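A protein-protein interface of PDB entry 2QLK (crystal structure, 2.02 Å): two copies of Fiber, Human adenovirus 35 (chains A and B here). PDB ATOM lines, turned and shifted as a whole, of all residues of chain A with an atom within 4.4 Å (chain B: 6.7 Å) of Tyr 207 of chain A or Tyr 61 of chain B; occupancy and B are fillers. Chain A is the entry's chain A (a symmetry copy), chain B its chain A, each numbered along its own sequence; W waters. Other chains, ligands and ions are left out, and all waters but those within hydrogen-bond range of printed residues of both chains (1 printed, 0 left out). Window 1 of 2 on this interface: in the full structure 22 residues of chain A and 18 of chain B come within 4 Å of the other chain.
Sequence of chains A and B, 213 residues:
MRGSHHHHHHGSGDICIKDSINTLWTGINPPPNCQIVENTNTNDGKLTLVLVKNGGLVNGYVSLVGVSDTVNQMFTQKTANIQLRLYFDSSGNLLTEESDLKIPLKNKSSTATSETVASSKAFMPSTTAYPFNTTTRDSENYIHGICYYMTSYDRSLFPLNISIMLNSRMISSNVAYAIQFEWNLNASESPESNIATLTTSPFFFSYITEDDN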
ATOM      1  N   LEU A  51      22.787  -8.494 -22.160  1.00  0.00           N
ATOM      2  CA  LEU A  51      22.232  -8.438 -20.816  1.00  0.00           C
ATOM      3  C   LEU A  51      21.696  -7.024 -20.572  1.00  0.00           C
ATOM      4  O   LEU A  51      22.426  -6.037 -20.699  1.00  0.00           O
ATOM      5  CB  LEU A  51      23.310  -8.763 -19.787  1.00  0.00           C
ATOM      6  CG  LEU A  51      23.997 -10.121 -19.892  1.00  0.00           C
ATOM      7  CD1 LEU A  51      25.156 -10.197 -18.933  1.00  0.00           C
ATOM      8  CD2 LEU A  51      22.973 -11.223 -19.531  1.00  0.00           C
ATOM      9  N   GLY A  56      14.746  -5.473 -10.764  1.00  0.00           N
ATOM     10  CA  GLY A  56      15.381  -6.568 -10.058  1.00  0.00           C
ATOM     11  C   GLY A  56      15.755  -7.722 -10.957  1.00  0.00           C
ATOM     12  O   GLY A  56      16.293  -8.728 -10.484  1.00  0.00           O
ATOM     13  N   LEU A  57      15.485  -7.569 -12.253  1.00  0.00           N
ATOM     14  CA  LEU A  57      15.761  -8.613 -13.239  1.00  0.00           C
ATOM     15  C   LEU A  57      16.688  -8.227 -14.362  1.00  0.00           C
ATOM     16  O   LEU A  57      16.646  -7.115 -14.842  1.00  0.00           O
ATOM     17  CB  LEU A  57      14.465  -9.031 -13.905  1.00  0.00           C
ATOM     18  CG  LEU A  57      13.808 -10.378 -13.625  1.00  0.00           C
ATOM     19  CD1 LEU A  57      14.005 -10.807 -12.186  1.00  0.00           C
ATOM     20  CD2 LEU A  57      12.341 -10.247 -14.012  1.00  0.00           C
ATOM     21  N   VAL A  58      17.525  -9.161 -14.786  1.00  0.00           N
ATOM     22  CA  VAL A  58      18.360  -8.920 -15.944  1.00  0.00           C
ATOM     23  C   VAL A  58      17.624  -9.662 -17.078  1.00  0.00           C
ATOM     24  O   VAL A  58      17.218 -10.817 -16.905  1.00  0.00           O
ATOM     25  CB  VAL A  58      19.767  -9.522 -15.785  1.00  0.00           C
ATOM     26  CG1 VAL A  58      20.519  -9.411 -17.088  1.00  0.00           C
ATOM     27  CG2 VAL A  58      20.529  -8.795 -14.693  1.00  0.00           C
ATOM     28  N   PHE A 123      24.581  -6.023 -13.242  1.00  0.00           N
ATOM     29  CA  PHE A 123      24.168  -6.969 -14.267  1.00  0.00           C
ATOM     30  C   PHE A 123      24.477  -8.386 -13.811  1.00  0.00           C
ATOM     31  O   PHE A 123      24.220  -9.344 -14.530  1.00  0.00           O
ATOM     32  CB  PHE A 123      24.921  -6.727 -15.576  1.00  0.00           C
ATOM     33  CG  PHE A 123      24.550  -5.459 -16.271  1.00  0.00           C
ATOM     34  CD1 PHE A 123      25.179  -4.253 -15.937  1.00  0.00           C
ATOM     35  CD2 PHE A 123      23.579  -5.465 -17.277  1.00  0.00           C
ATOM     36  CE1 PHE A 123      24.847  -3.062 -16.603  1.00  0.00           C
ATOM     37  CE2 PHE A 123      23.232  -4.297 -17.952  1.00  0.00           C
ATOM     38  CZ  PHE A 123      23.871  -3.079 -17.615  1.00  0.00           C
ATOM     39  N   MET A 124      25.028  -8.521 -12.613  1.00  0.00           N
ATOM     40  CA  MET A 124      25.419  -9.828 -12.109  1.00  0.00           C
ATOM     41  C   MET A 124      24.311 -10.570 -11.383  1.00  0.00           C
ATOM     42  O   MET A 124      23.403  -9.954 -10.821  1.00  0.00           O
ATOM     43  CB  MET A 124      26.617  -9.664 -11.172  1.00  0.00           C
ATOM     44  CG  MET A 124      27.851  -9.062 -11.835  1.00  0.00           C
ATOM     45  SD  MET A 124      28.678 -10.245 -12.975  1.00  0.00           S
ATOM     46  CE  MET A 124      28.402  -9.470 -14.474  1.00  0.00           C
ATOM     47  N   PRO A 125      24.357 -11.908 -11.414  1.00  0.00           N
ATOM     48  CA  PRO A 125      23.386 -12.791 -10.764  1.00  0.00           C
ATOM     49  C   PRO A 125      23.514 -12.758  -9.248  1.00  0.00           C
ATOM     50  O   PRO A 125      24.582 -13.083  -8.689  1.00  0.00           O
ATOM     51  CB  PRO A 125      23.749 -14.177 -11.304  1.00  0.00           C
ATOM     52  CG  PRO A 125      25.226 -14.036 -11.611  1.00  0.00           C
ATOM     53  CD  PRO A 125      25.275 -12.687 -12.263  1.00  0.00           C
ATOM     54  N   TYR A 130      21.075 -16.954  -6.186  1.00  0.00           N
ATOM     55  CA  TYR A 130      21.868 -18.069  -6.726  1.00  0.00           C
ATOM     56  C   TYR A 130      23.182 -18.199  -5.952  1.00  0.00           C
ATOM     57  O   TYR A 130      24.227 -17.673  -6.362  1.00  0.00           O
ATOM     58  CB  TYR A 130      22.129 -17.817  -8.213  1.00  0.00           C
ATOM     59  CG  TYR A 130      20.886 -17.273  -8.901  1.00  0.00           C
ATOM     60  CD1 TYR A 130      19.720 -18.041  -9.002  1.00  0.00           C
ATOM     61  CD2 TYR A 130      20.863 -15.973  -9.401  1.00  0.00           C
ATOM     62  CE1 TYR A 130      18.546 -17.518  -9.588  1.00  0.00           C
ATOM     63  CE2 TYR A 130      19.716 -15.447  -9.970  1.00  0.00           C
ATOM     64  CZ  TYR A 130      18.560 -16.221 -10.059  1.00  0.00           C
ATOM     65  OH  TYR A 130      17.439 -15.655 -10.601  1.00  0.00           O
ATOM     66  N   LEU A 166      23.868 -20.366 -12.840  1.00  0.00           N
ATOM     67  CA  LEU A 166      24.296 -19.110 -12.242  1.00  0.00           C
ATOM     68  C   LEU A 166      25.165 -19.319 -11.011  1.00  0.00           C
ATOM     69  O   LEU A 166      24.811 -20.091 -10.120  1.00  0.00           O
ATOM     70  CB  LEU A 166      23.065 -18.252 -11.893  1.00  0.00           C
ATOM     71  CG  LEU A 166      22.111 -18.022 -13.079  1.00  0.00           C
ATOM     72  CD1 LEU A 166      20.777 -17.549 -12.544  1.00  0.00           C
ATOM     73  CD2 LEU A 166      22.709 -17.033 -14.104  1.00  0.00           C
ATOM     74  N   ILE A 179      28.432 -17.339 -14.839  1.00  0.00           N
ATOM     75  CA  ILE A 179      27.332 -17.608 -15.747  1.00  0.00           C
ATOM     76  C   ILE A 179      27.913 -18.627 -16.717  1.00  0.00           C
ATOM     77  O   ILE A 179      28.910 -18.346 -17.408  1.00  0.00           O
ATOM     78  CB  ILE A 179      26.924 -16.366 -16.542  1.00  0.00           C
ATOM     79  CG1 ILE A 179      26.456 -15.269 -15.589  1.00  0.00           C
ATOM     80  CG2 ILE A 179      25.812 -16.736 -17.549  1.00  0.00           C
ATOM     81  CD1 ILE A 179      25.906 -14.035 -16.299  1.00  0.00           C
ATOM     82  N   PHE A 205      16.102 -15.244 -21.572  1.00  0.00           N
ATOM     83  CA  PHE A 205      16.007 -15.626 -20.162  1.00  0.00           C
ATOM     84  C   PHE A 205      16.072 -14.396 -19.281  1.00  0.00           C
ATOM     85  O   PHE A 205      16.320 -13.287 -19.764  1.00  0.00           O
ATOM     86  CB  PHE A 205      17.178 -16.544 -19.789  1.00  0.00           C
ATOM     87  CG  PHE A 205      18.540 -15.926 -20.051  1.00  0.00           C
ATOM     88  CD1 PHE A 205      19.067 -15.892 -21.336  1.00  0.00           C
ATOM     89  CD2 PHE A 205      19.286 -15.376 -19.009  1.00  0.00           C
ATOM     90  CE1 PHE A 205      20.305 -15.334 -21.600  1.00  0.00           C
ATOM     91  CE2 PHE A 205      20.529 -14.812 -19.253  1.00  0.00           C
ATOM     92  CZ  PHE A 205      21.047 -14.790 -20.561  1.00  0.00           C
ATOM     93  N   SER A 206      15.815 -14.596 -17.997  1.00  0.00           N
ATOM     94  CA  SER A 206      15.936 -13.521 -17.036  1.00  0.00           C
ATOM     95  C   SER A 206      16.476 -14.137 -15.743  1.00  0.00           C
ATOM     96  O   SER A 206      16.334 -15.356 -15.507  1.00  0.00           O
ATOM     97  CB  SER A 206      14.589 -12.870 -16.738  1.00  0.00           C
ATOM     98  OG  SER A 206      13.947 -12.425 -17.920  1.00  0.00           O
ATOM     99  N   TYR A 207      17.133 -13.307 -14.935  1.00  0.00           N
ATOM    100  CA  TYR A 207      17.606 -13.728 -13.624  1.00  0.00           C
ATOM    101  C   TYR A 207      17.607 -12.514 -12.688  1.00  0.00           C
ATOM    102  O   TYR A 207      17.622 -11.374 -13.124  1.00  0.00           O
ATOM    103  CB  TYR A 207      18.988 -14.425 -13.674  1.00  0.00           C
ATOM    104  CG  TYR A 207      20.144 -13.636 -14.252  1.00  0.00           C
ATOM    105  CD1 TYR A 207      20.760 -12.609 -13.531  1.00  0.00           C
ATOM    106  CD2 TYR A 207      20.635 -13.938 -15.520  1.00  0.00           C
ATOM    107  CE1 TYR A 207      21.860 -11.901 -14.071  1.00  0.00           C
ATOM    108  CE2 TYR A 207      21.725 -13.237 -16.075  1.00  0.00           C
ATOM    109  CZ  TYR A 207      22.333 -12.226 -15.348  1.00  0.00           C
ATOM    110  OH  TYR A 207      23.421 -11.573 -15.897  1.00  0.00           O
ATOM    111  N   ILE A 208      17.521 -12.791 -11.403  1.00  0.00           N
ATOM    112  CA  ILE A 208      17.478 -11.780 -10.364  1.00  0.00           C
ATOM    113  C   ILE A 208      18.878 -11.193 -10.194  1.00  0.00           C
ATOM    114  O   ILE A 208      19.862 -11.917 -10.014  1.00  0.00           O
ATOM    115  CB  ILE A 208      17.002 -12.421  -9.067  1.00  0.00           C
ATOM    116  CG1 ILE A 208      15.620 -13.034  -9.309  1.00  0.00           C
ATOM    117  CG2 ILE A 208      16.978 -11.368  -7.922  1.00  0.00           C
ATOM    118  CD1 ILE A 208      15.109 -13.874  -8.153  1.00  0.00           C
ATOM    119  N   THR A 209      18.951  -9.877 -10.278  1.00  0.00           N
ATOM    120  CA  THR A 209      20.224  -9.196 -10.180  1.00  0.00           C
ATOM    121  C   THR A 209      20.628  -8.843  -8.766  1.00  0.00           C
ATOM    122  O   THR A 209      19.787  -8.753  -7.875  1.00  0.00           O
ATOM    123  CB  THR A 209      20.223  -7.909 -11.015  1.00  0.00           C
ATOM    124  OG1 THR A 209      21.531  -7.331 -10.974  1.00  0.00           O
ATOM    125  CG2 THR A 209      19.217  -6.906 -10.467  1.00  0.00           C
ATOM    126  N   THR B  48       9.035 -17.567  -5.466  1.00  0.00           N
ATOM    127  CA  THR B  48       9.825 -16.397  -5.850  1.00  0.00           C
ATOM    128  C   THR B  48       9.154 -15.880  -7.120  1.00  0.00           C
ATOM    129  O   THR B  48       9.156 -16.540  -8.175  1.00  0.00           O
ATOM    130  CB  THR B  48      11.283 -16.761  -6.187  1.00  0.00           C
ATOM    131  OG1 THR B  48      11.922 -17.296  -5.021  1.00  0.00           O
ATOM    132  CG2 THR B  48      12.054 -15.527  -6.699  1.00  0.00           C
ATOM    133  N   LEU B  49       8.565 -14.703  -7.007  1.00  0.00           N
ATOM    134  CA  LEU B  49       7.892 -14.079  -8.110  1.00  0.00           C
ATOM    135  C   LEU B  49       8.455 -12.682  -8.229  1.00  0.00           C
ATOM    136  O   LEU B  49       8.494 -11.954  -7.239  1.00  0.00           O
ATOM    137  CB  LEU B  49       6.404 -13.975  -7.824  1.00  0.00           C
ATOM    138  CG  LEU B  49       5.586 -13.145  -8.810  1.00  0.00           C
ATOM    139  CD1 LEU B  49       5.550 -13.810 -10.202  1.00  0.00           C
ATOM    140  CD2 LEU B  49       4.185 -13.028  -8.245  1.00  0.00           C
ATOM    141  N   VAL B  50       8.904 -12.325  -9.427  1.00  0.00           N
ATOM    142  CA  VAL B  50       9.426 -11.017  -9.692  1.00  0.00           C
ATOM    143  C   VAL B  50       8.659 -10.429 -10.879  1.00  0.00           C
ATOM    144  O   VAL B  50       8.625 -11.010 -11.961  1.00  0.00           O
ATOM    145  CB  VAL B  50      10.908 -11.104  -9.983  1.00  0.00           C
ATOM    146  CG1 VAL B  50      11.509  -9.688 -10.076  1.00  0.00           C
ATOM    147  CG2 VAL B  50      11.592 -11.911  -8.871  1.00  0.00           C
ATOM    148  N   LEU B  51       8.020  -9.285 -10.652  1.00  0.00           N
ATOM    149  CA  LEU B  51       7.262  -8.580 -11.676  1.00  0.00           C
ATOM    150  C   LEU B  51       7.923  -7.219 -11.916  1.00  0.00           C
ATOM    151  O   LEU B  51       8.096  -6.425 -10.987  1.00  0.00           O
ATOM    152  CB  LEU B  51       5.821  -8.378 -11.218  1.00  0.00           C
ATOM    153  CG  LEU B  51       5.005  -9.625 -10.888  1.00  0.00           C
ATOM    154  CD1 LEU B  51       3.687  -9.240 -10.272  1.00  0.00           C
ATOM    155  CD2 LEU B  51       4.741 -10.404 -12.197  1.00  0.00           C
ATOM    156  N   VAL B  52       8.315  -6.973 -13.163  1.00  0.00           N
ATOM    157  CA  VAL B  52       8.956  -5.728 -13.543  1.00  0.00           C
ATOM    158  C   VAL B  52       8.113  -4.965 -14.568  1.00  0.00           C
ATOM    159  O   VAL B  52       7.731  -5.515 -15.614  1.00  0.00           O
ATOM    160  CB  VAL B  52      10.351  -5.980 -14.156  1.00  0.00           C
ATOM    161  CG1 VAL B  52      10.892  -4.682 -14.764  1.00  0.00           C
ATOM    162  CG2 VAL B  52      11.309  -6.528 -13.104  1.00  0.00           C
ATOM    163  N   ASN B  59       7.265  -7.748 -17.127  1.00  0.00           N
ATOM    164  CA  ASN B  59       8.210  -8.833 -17.368  1.00  0.00           C
ATOM    165  C   ASN B  59       8.250  -9.649 -16.088  1.00  0.00           C
ATOM    166  O   ASN B  59       8.600  -9.134 -15.028  1.00  0.00           O
ATOM    167  CB  ASN B  59       9.606  -8.298 -17.688  1.00  0.00           C
ATOM    168  CG  ASN B  59       9.800  -8.017 -19.167  1.00  0.00           C
ATOM    169  OD1 ASN B  59       8.838  -7.987 -19.944  1.00  0.00           O
ATOM    170  ND2 ASN B  59      11.046  -7.800 -19.567  1.00  0.00           N
ATOM    171  N   GLY B  60       7.886 -10.919 -16.176  1.00  0.00           N
ATOM    172  CA  GLY B  60       7.866 -11.740 -14.984  1.00  0.00           C
ATOM    173  C   GLY B  60       8.806 -12.920 -14.900  1.00  0.00           C
ATOM    174  O   GLY B  60       9.290 -13.444 -15.910  1.00  0.00           O
ATOM    175  N   TYR B  61       9.033 -13.346 -13.664  1.00  0.00           N
ATOM    176  CA  TYR B  61       9.899 -14.469 -13.360  1.00  0.00           C
ATOM    177  C   TYR B  61       9.269 -15.225 -12.199  1.00  0.00           C
ATOM    178  O   TYR B  61       8.930 -14.649 -11.148  1.00  0.00           O
ATOM    179  CB  TYR B  61      11.282 -13.923 -13.019  1.00  0.00           C
ATOM    180  CG  TYR B  61      12.309 -14.879 -12.500  1.00  0.00           C
ATOM    181  CD1 TYR B  61      12.122 -15.528 -11.275  1.00  0.00           C
ATOM    182  CD2 TYR B  61      13.505 -15.064 -13.168  1.00  0.00           C
ATOM    183  CE1 TYR B  61      13.115 -16.333 -10.721  1.00  0.00           C
ATOM    184  CE2 TYR B  61      14.516 -15.884 -12.631  1.00  0.00           C
ATOM    185  CZ  TYR B  61      14.310 -16.505 -11.409  1.00  0.00           C
ATOM    186  OH  TYR B  61      15.291 -17.268 -10.842  1.00  0.00           O
ATOM    187  N   VAL B  62       9.112 -16.530 -12.362  1.00  0.00           N
ATOM    188  CA  VAL B  62       8.503 -17.291 -11.308  1.00  0.00           C
ATOM    189  C   VAL B  62       9.128 -18.666 -11.083  1.00  0.00           C
ATOM    190  O   VAL B  62       9.334 -19.437 -12.016  1.00  0.00           O
ATOM    191  CB  VAL B  62       6.952 -17.402 -11.549  1.00  0.00           C
ATOM    192  CG1 VAL B  62       6.643 -18.236 -12.806  1.00  0.00           C
ATOM    193  CG2 VAL B  62       6.258 -18.006 -10.302  1.00  0.00           C
ATOM    194  N   SER B  63       9.449 -18.958  -9.829  1.00  0.00           N
ATOM    195  CA  SER B  63      10.006 -20.263  -9.489  1.00  0.00           C
ATOM    196  C   SER B  63       9.468 -20.600  -8.121  1.00  0.00           C
ATOM    197  O   SER B  63       9.148 -19.708  -7.321  1.00  0.00           O
ATOM    198  CB  SER B  63      11.548 -20.287  -9.480  1.00  0.00           C
ATOM    199  OG  SER B  63      12.056 -19.509  -8.431  1.00  0.00           O
ATOM    200  N   PHE B 181      -1.134 -19.448 -10.976  1.00  0.00           N
ATOM    201  CA  PHE B 181      -0.030 -20.224 -11.548  1.00  0.00           C
ATOM    202  C   PHE B 181      -0.370 -21.675 -11.355  1.00  0.00           C
ATOM    203  O   PHE B 181      -0.859 -22.063 -10.294  1.00  0.00           O
ATOM    204  CB  PHE B 181       1.287 -19.955 -10.789  1.00  0.00           C
ATOM    205  CG  PHE B 181       1.817 -18.551 -10.929  1.00  0.00           C
ATOM    206  CD1 PHE B 181       2.542 -18.166 -12.070  1.00  0.00           C
ATOM    207  CD2 PHE B 181       1.566 -17.606  -9.946  1.00  0.00           C
ATOM    208  CE1 PHE B 181       3.002 -16.841 -12.221  1.00  0.00           C
ATOM    209  CE2 PHE B 181       2.020 -16.278 -10.085  1.00  0.00           C
ATOM    210  CZ  PHE B 181       2.736 -15.893 -11.224  1.00  0.00           C
ATOM    211  N   PRO B 202      12.935 -21.726 -13.199  1.00  0.00           N
ATOM    212  CA  PRO B 202      12.335 -20.434 -13.539  1.00  0.00           C
ATOM    213  C   PRO B 202      11.605 -20.343 -14.885  1.00  0.00           C
ATOM    214  O   PRO B 202      12.142 -20.711 -15.934  1.00  0.00           O
ATOM    215  CB  PRO B 202      13.529 -19.463 -13.485  1.00  0.00           C
ATOM    216  CG  PRO B 202      14.546 -20.174 -12.669  1.00  0.00           C
ATOM    217  CD  PRO B 202      14.392 -21.613 -13.040  1.00  0.00           C
ATOM    218  N   PHE B 203      10.375 -19.833 -14.837  1.00  0.00           N
ATOM    219  CA  PHE B 203       9.566 -19.631 -16.037  1.00  0.00           C
ATOM    220  C   PHE B 203       9.442 -18.119 -16.258  1.00  0.00           C
ATOM    221  O   PHE B 203       9.052 -17.372 -15.339  1.00  0.00           O
ATOM    222  CB  PHE B 203       8.169 -20.232 -15.873  1.00  0.00           C
ATOM    223  CG  PHE B 203       7.293 -20.060 -17.089  1.00  0.00           C
ATOM    224  CD1 PHE B 203       7.613 -20.682 -18.300  1.00  0.00           C
ATOM    225  CD2 PHE B 203       6.183 -19.204 -17.054  1.00  0.00           C
ATOM    226  CE1 PHE B 203       6.842 -20.439 -19.473  1.00  0.00           C
ATOM    227  CE2 PHE B 203       5.411 -18.961 -18.217  1.00  0.00           C
ATOM    228  CZ  PHE B 203       5.745 -19.572 -19.417  1.00  0.00           C
ATOM    229  N   PHE B 204       9.752 -17.686 -17.483  1.00  0.00           N
ATOM    230  CA  PHE B 204       9.699 -16.286 -17.839  1.00  0.00           C
ATOM    231  C   PHE B 204       8.462 -15.979 -18.652  1.00  0.00           C
ATOM    232  O   PHE B 204       8.076 -16.742 -19.542  1.00  0.00           O
ATOM    233  CB  PHE B 204      10.924 -15.906 -18.647  1.00  0.00           C
ATOM    234  CG  PHE B 204      12.173 -16.527 -18.161  1.00  0.00           C
ATOM    235  CD1 PHE B 204      12.584 -16.346 -16.867  1.00  0.00           C
ATOM    236  CD2 PHE B 204      12.951 -17.298 -19.012  1.00  0.00           C
ATOM    237  CE1 PHE B 204      13.747 -16.911 -16.417  1.00  0.00           C
ATOM    238  CE2 PHE B 204      14.115 -17.863 -18.566  1.00  0.00           C
ATOM    239  CZ  PHE B 204      14.519 -17.667 -17.260  1.00  0.00           C
ATOM    240  N   PHE B 205       7.846 -14.839 -18.381  1.00  0.00           N
ATOM    241  CA  PHE B 205       6.635 -14.491 -19.127  1.00  0.00           C
ATOM    242  C   PHE B 205       6.442 -12.989 -19.139  1.00  0.00           C
ATOM    243  O   PHE B 205       7.169 -12.254 -18.463  1.00  0.00           O
ATOM    244  CB  PHE B 205       5.409 -15.126 -18.460  1.00  0.00           C
ATOM    245  CG  PHE B 205       5.234 -14.726 -17.005  1.00  0.00           C
ATOM    246  CD1 PHE B 205       5.998 -15.323 -16.010  1.00  0.00           C
ATOM    247  CD2 PHE B 205       4.309 -13.749 -16.641  1.00  0.00           C
ATOM    248  CE1 PHE B 205       5.859 -14.975 -14.679  1.00  0.00           C
ATOM    249  CE2 PHE B 205       4.153 -13.386 -15.312  1.00  0.00           C
ATOM    250  CZ  PHE B 205       4.934 -14.005 -14.318  1.00  0.00           C
HETATM  251  O   HOH W   1      11.222 -12.297 -17.566  1.00  0.00           O
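The side-chain hydroxyl of Tyr 61 of chain B lies within hydrogen-bond range of the side-chain hydroxyl of Tyr 130 of chain A, at 2.7 Å.
The backbone carbonyl oxygen (O) of Ser 63 of chain B lies within hydrogen-bond range of the backbone NH (N) of Thr 48 of chain B, 2.8 Å away.
The backbone carbonyl oxygen of Tyr 61 of chain B sits at hydrogen-bond distance from the backbone NH of Val 50 of chain B, at 2.9 Å.
The backbone carbonyl oxygen (O) of Val 52 of chain B sits at hydrogen-bond distance from the backbone NH (N) of Asn 59 of chain B, 2.7 Å away.
O of Tyr 207 of chain A is in hydrogen-bond range of N of Val 58 of chain A.
OH of Tyr 207 of chain A lies within hydrogen-bond range of O of Phe 123 of chain A (2.7 Å).
OH of Tyr 130 of chain A is in hydrogen-bond range of N of Ile 208 of chain A, 3.0 Å away.
Among the printed residues, merely in contact across the chains: Ser 206 of chain A with Phe 204 of chain B (3.2 Å), Phe 205 of chain A with Phe 204 of chain B (3.3 Å), Ser 206 of chain A with Tyr 61 of chain B (3.4 Å), Leu 57 of chain A with Val 50 of chain B (3.5 Å), Ile 208 of chain A with Thr 48 of chain B (3.8 Å), Tyr 207 of chain A with Tyr 61 of chain B (3.9 Å), Leu 57 of chain A with Tyr 61 of chain B (3.95 Å) and Leu 57 of chain A with Val 52 of chain B (3.96 Å).
Of chain B, only Tyr 61 (3.9 Å) comes within 4 Å of Tyr 207 of chain A.
Tyr 61 of chain B touches just these residues of chain A: Leu 57 (3.95 Å), Tyr 130 (2.7 Å), Ser 206 (3.4 Å) and Tyr 207 (3.9 Å).
Printed residues of chain B within 4 Å of Leu 57 of chain A: Val 50, Val 52 and Tyr 61.
Printed residues of chain A within 4 Å of Val 52 of chain B: Leu 57 (3.96 Å).
Of the printed residues of chain B, Phe 205 of chain A touches Phe 204.
Of the printed residues of chain B, Ile 208 of chain A touches Thr 48.
Of the printed residues of chain A, Phe 204 of chain B touches Phe 205 (3.3 Å) and Ser 206 (3.2 Å).
Ser 63 of chain B touches none of the printed residues of chain A.
Leu 51 of chain B touches none of the printed residues of chain A.
The nearest printed residue of chain A that does not touch Val 50 of chain B is Ile 208 of chain A (4.1 Å).
Of the 15 printed residues of chain B, 5 touch a printed residue of chain A.
Positions printed for both chains: 51 and 205.
Of the 9 pairs that touch across the chains among the printed residues, none has its exchanged pair printed and touching as well.
Water W1 lies within hydrogen-bond range of the side-chain hydroxyl (OG) of Ser 206 of chain A (2.8 Å) and the backbone carbonyl oxygen (O) of Gly 60 of chain B (2.8 Å).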
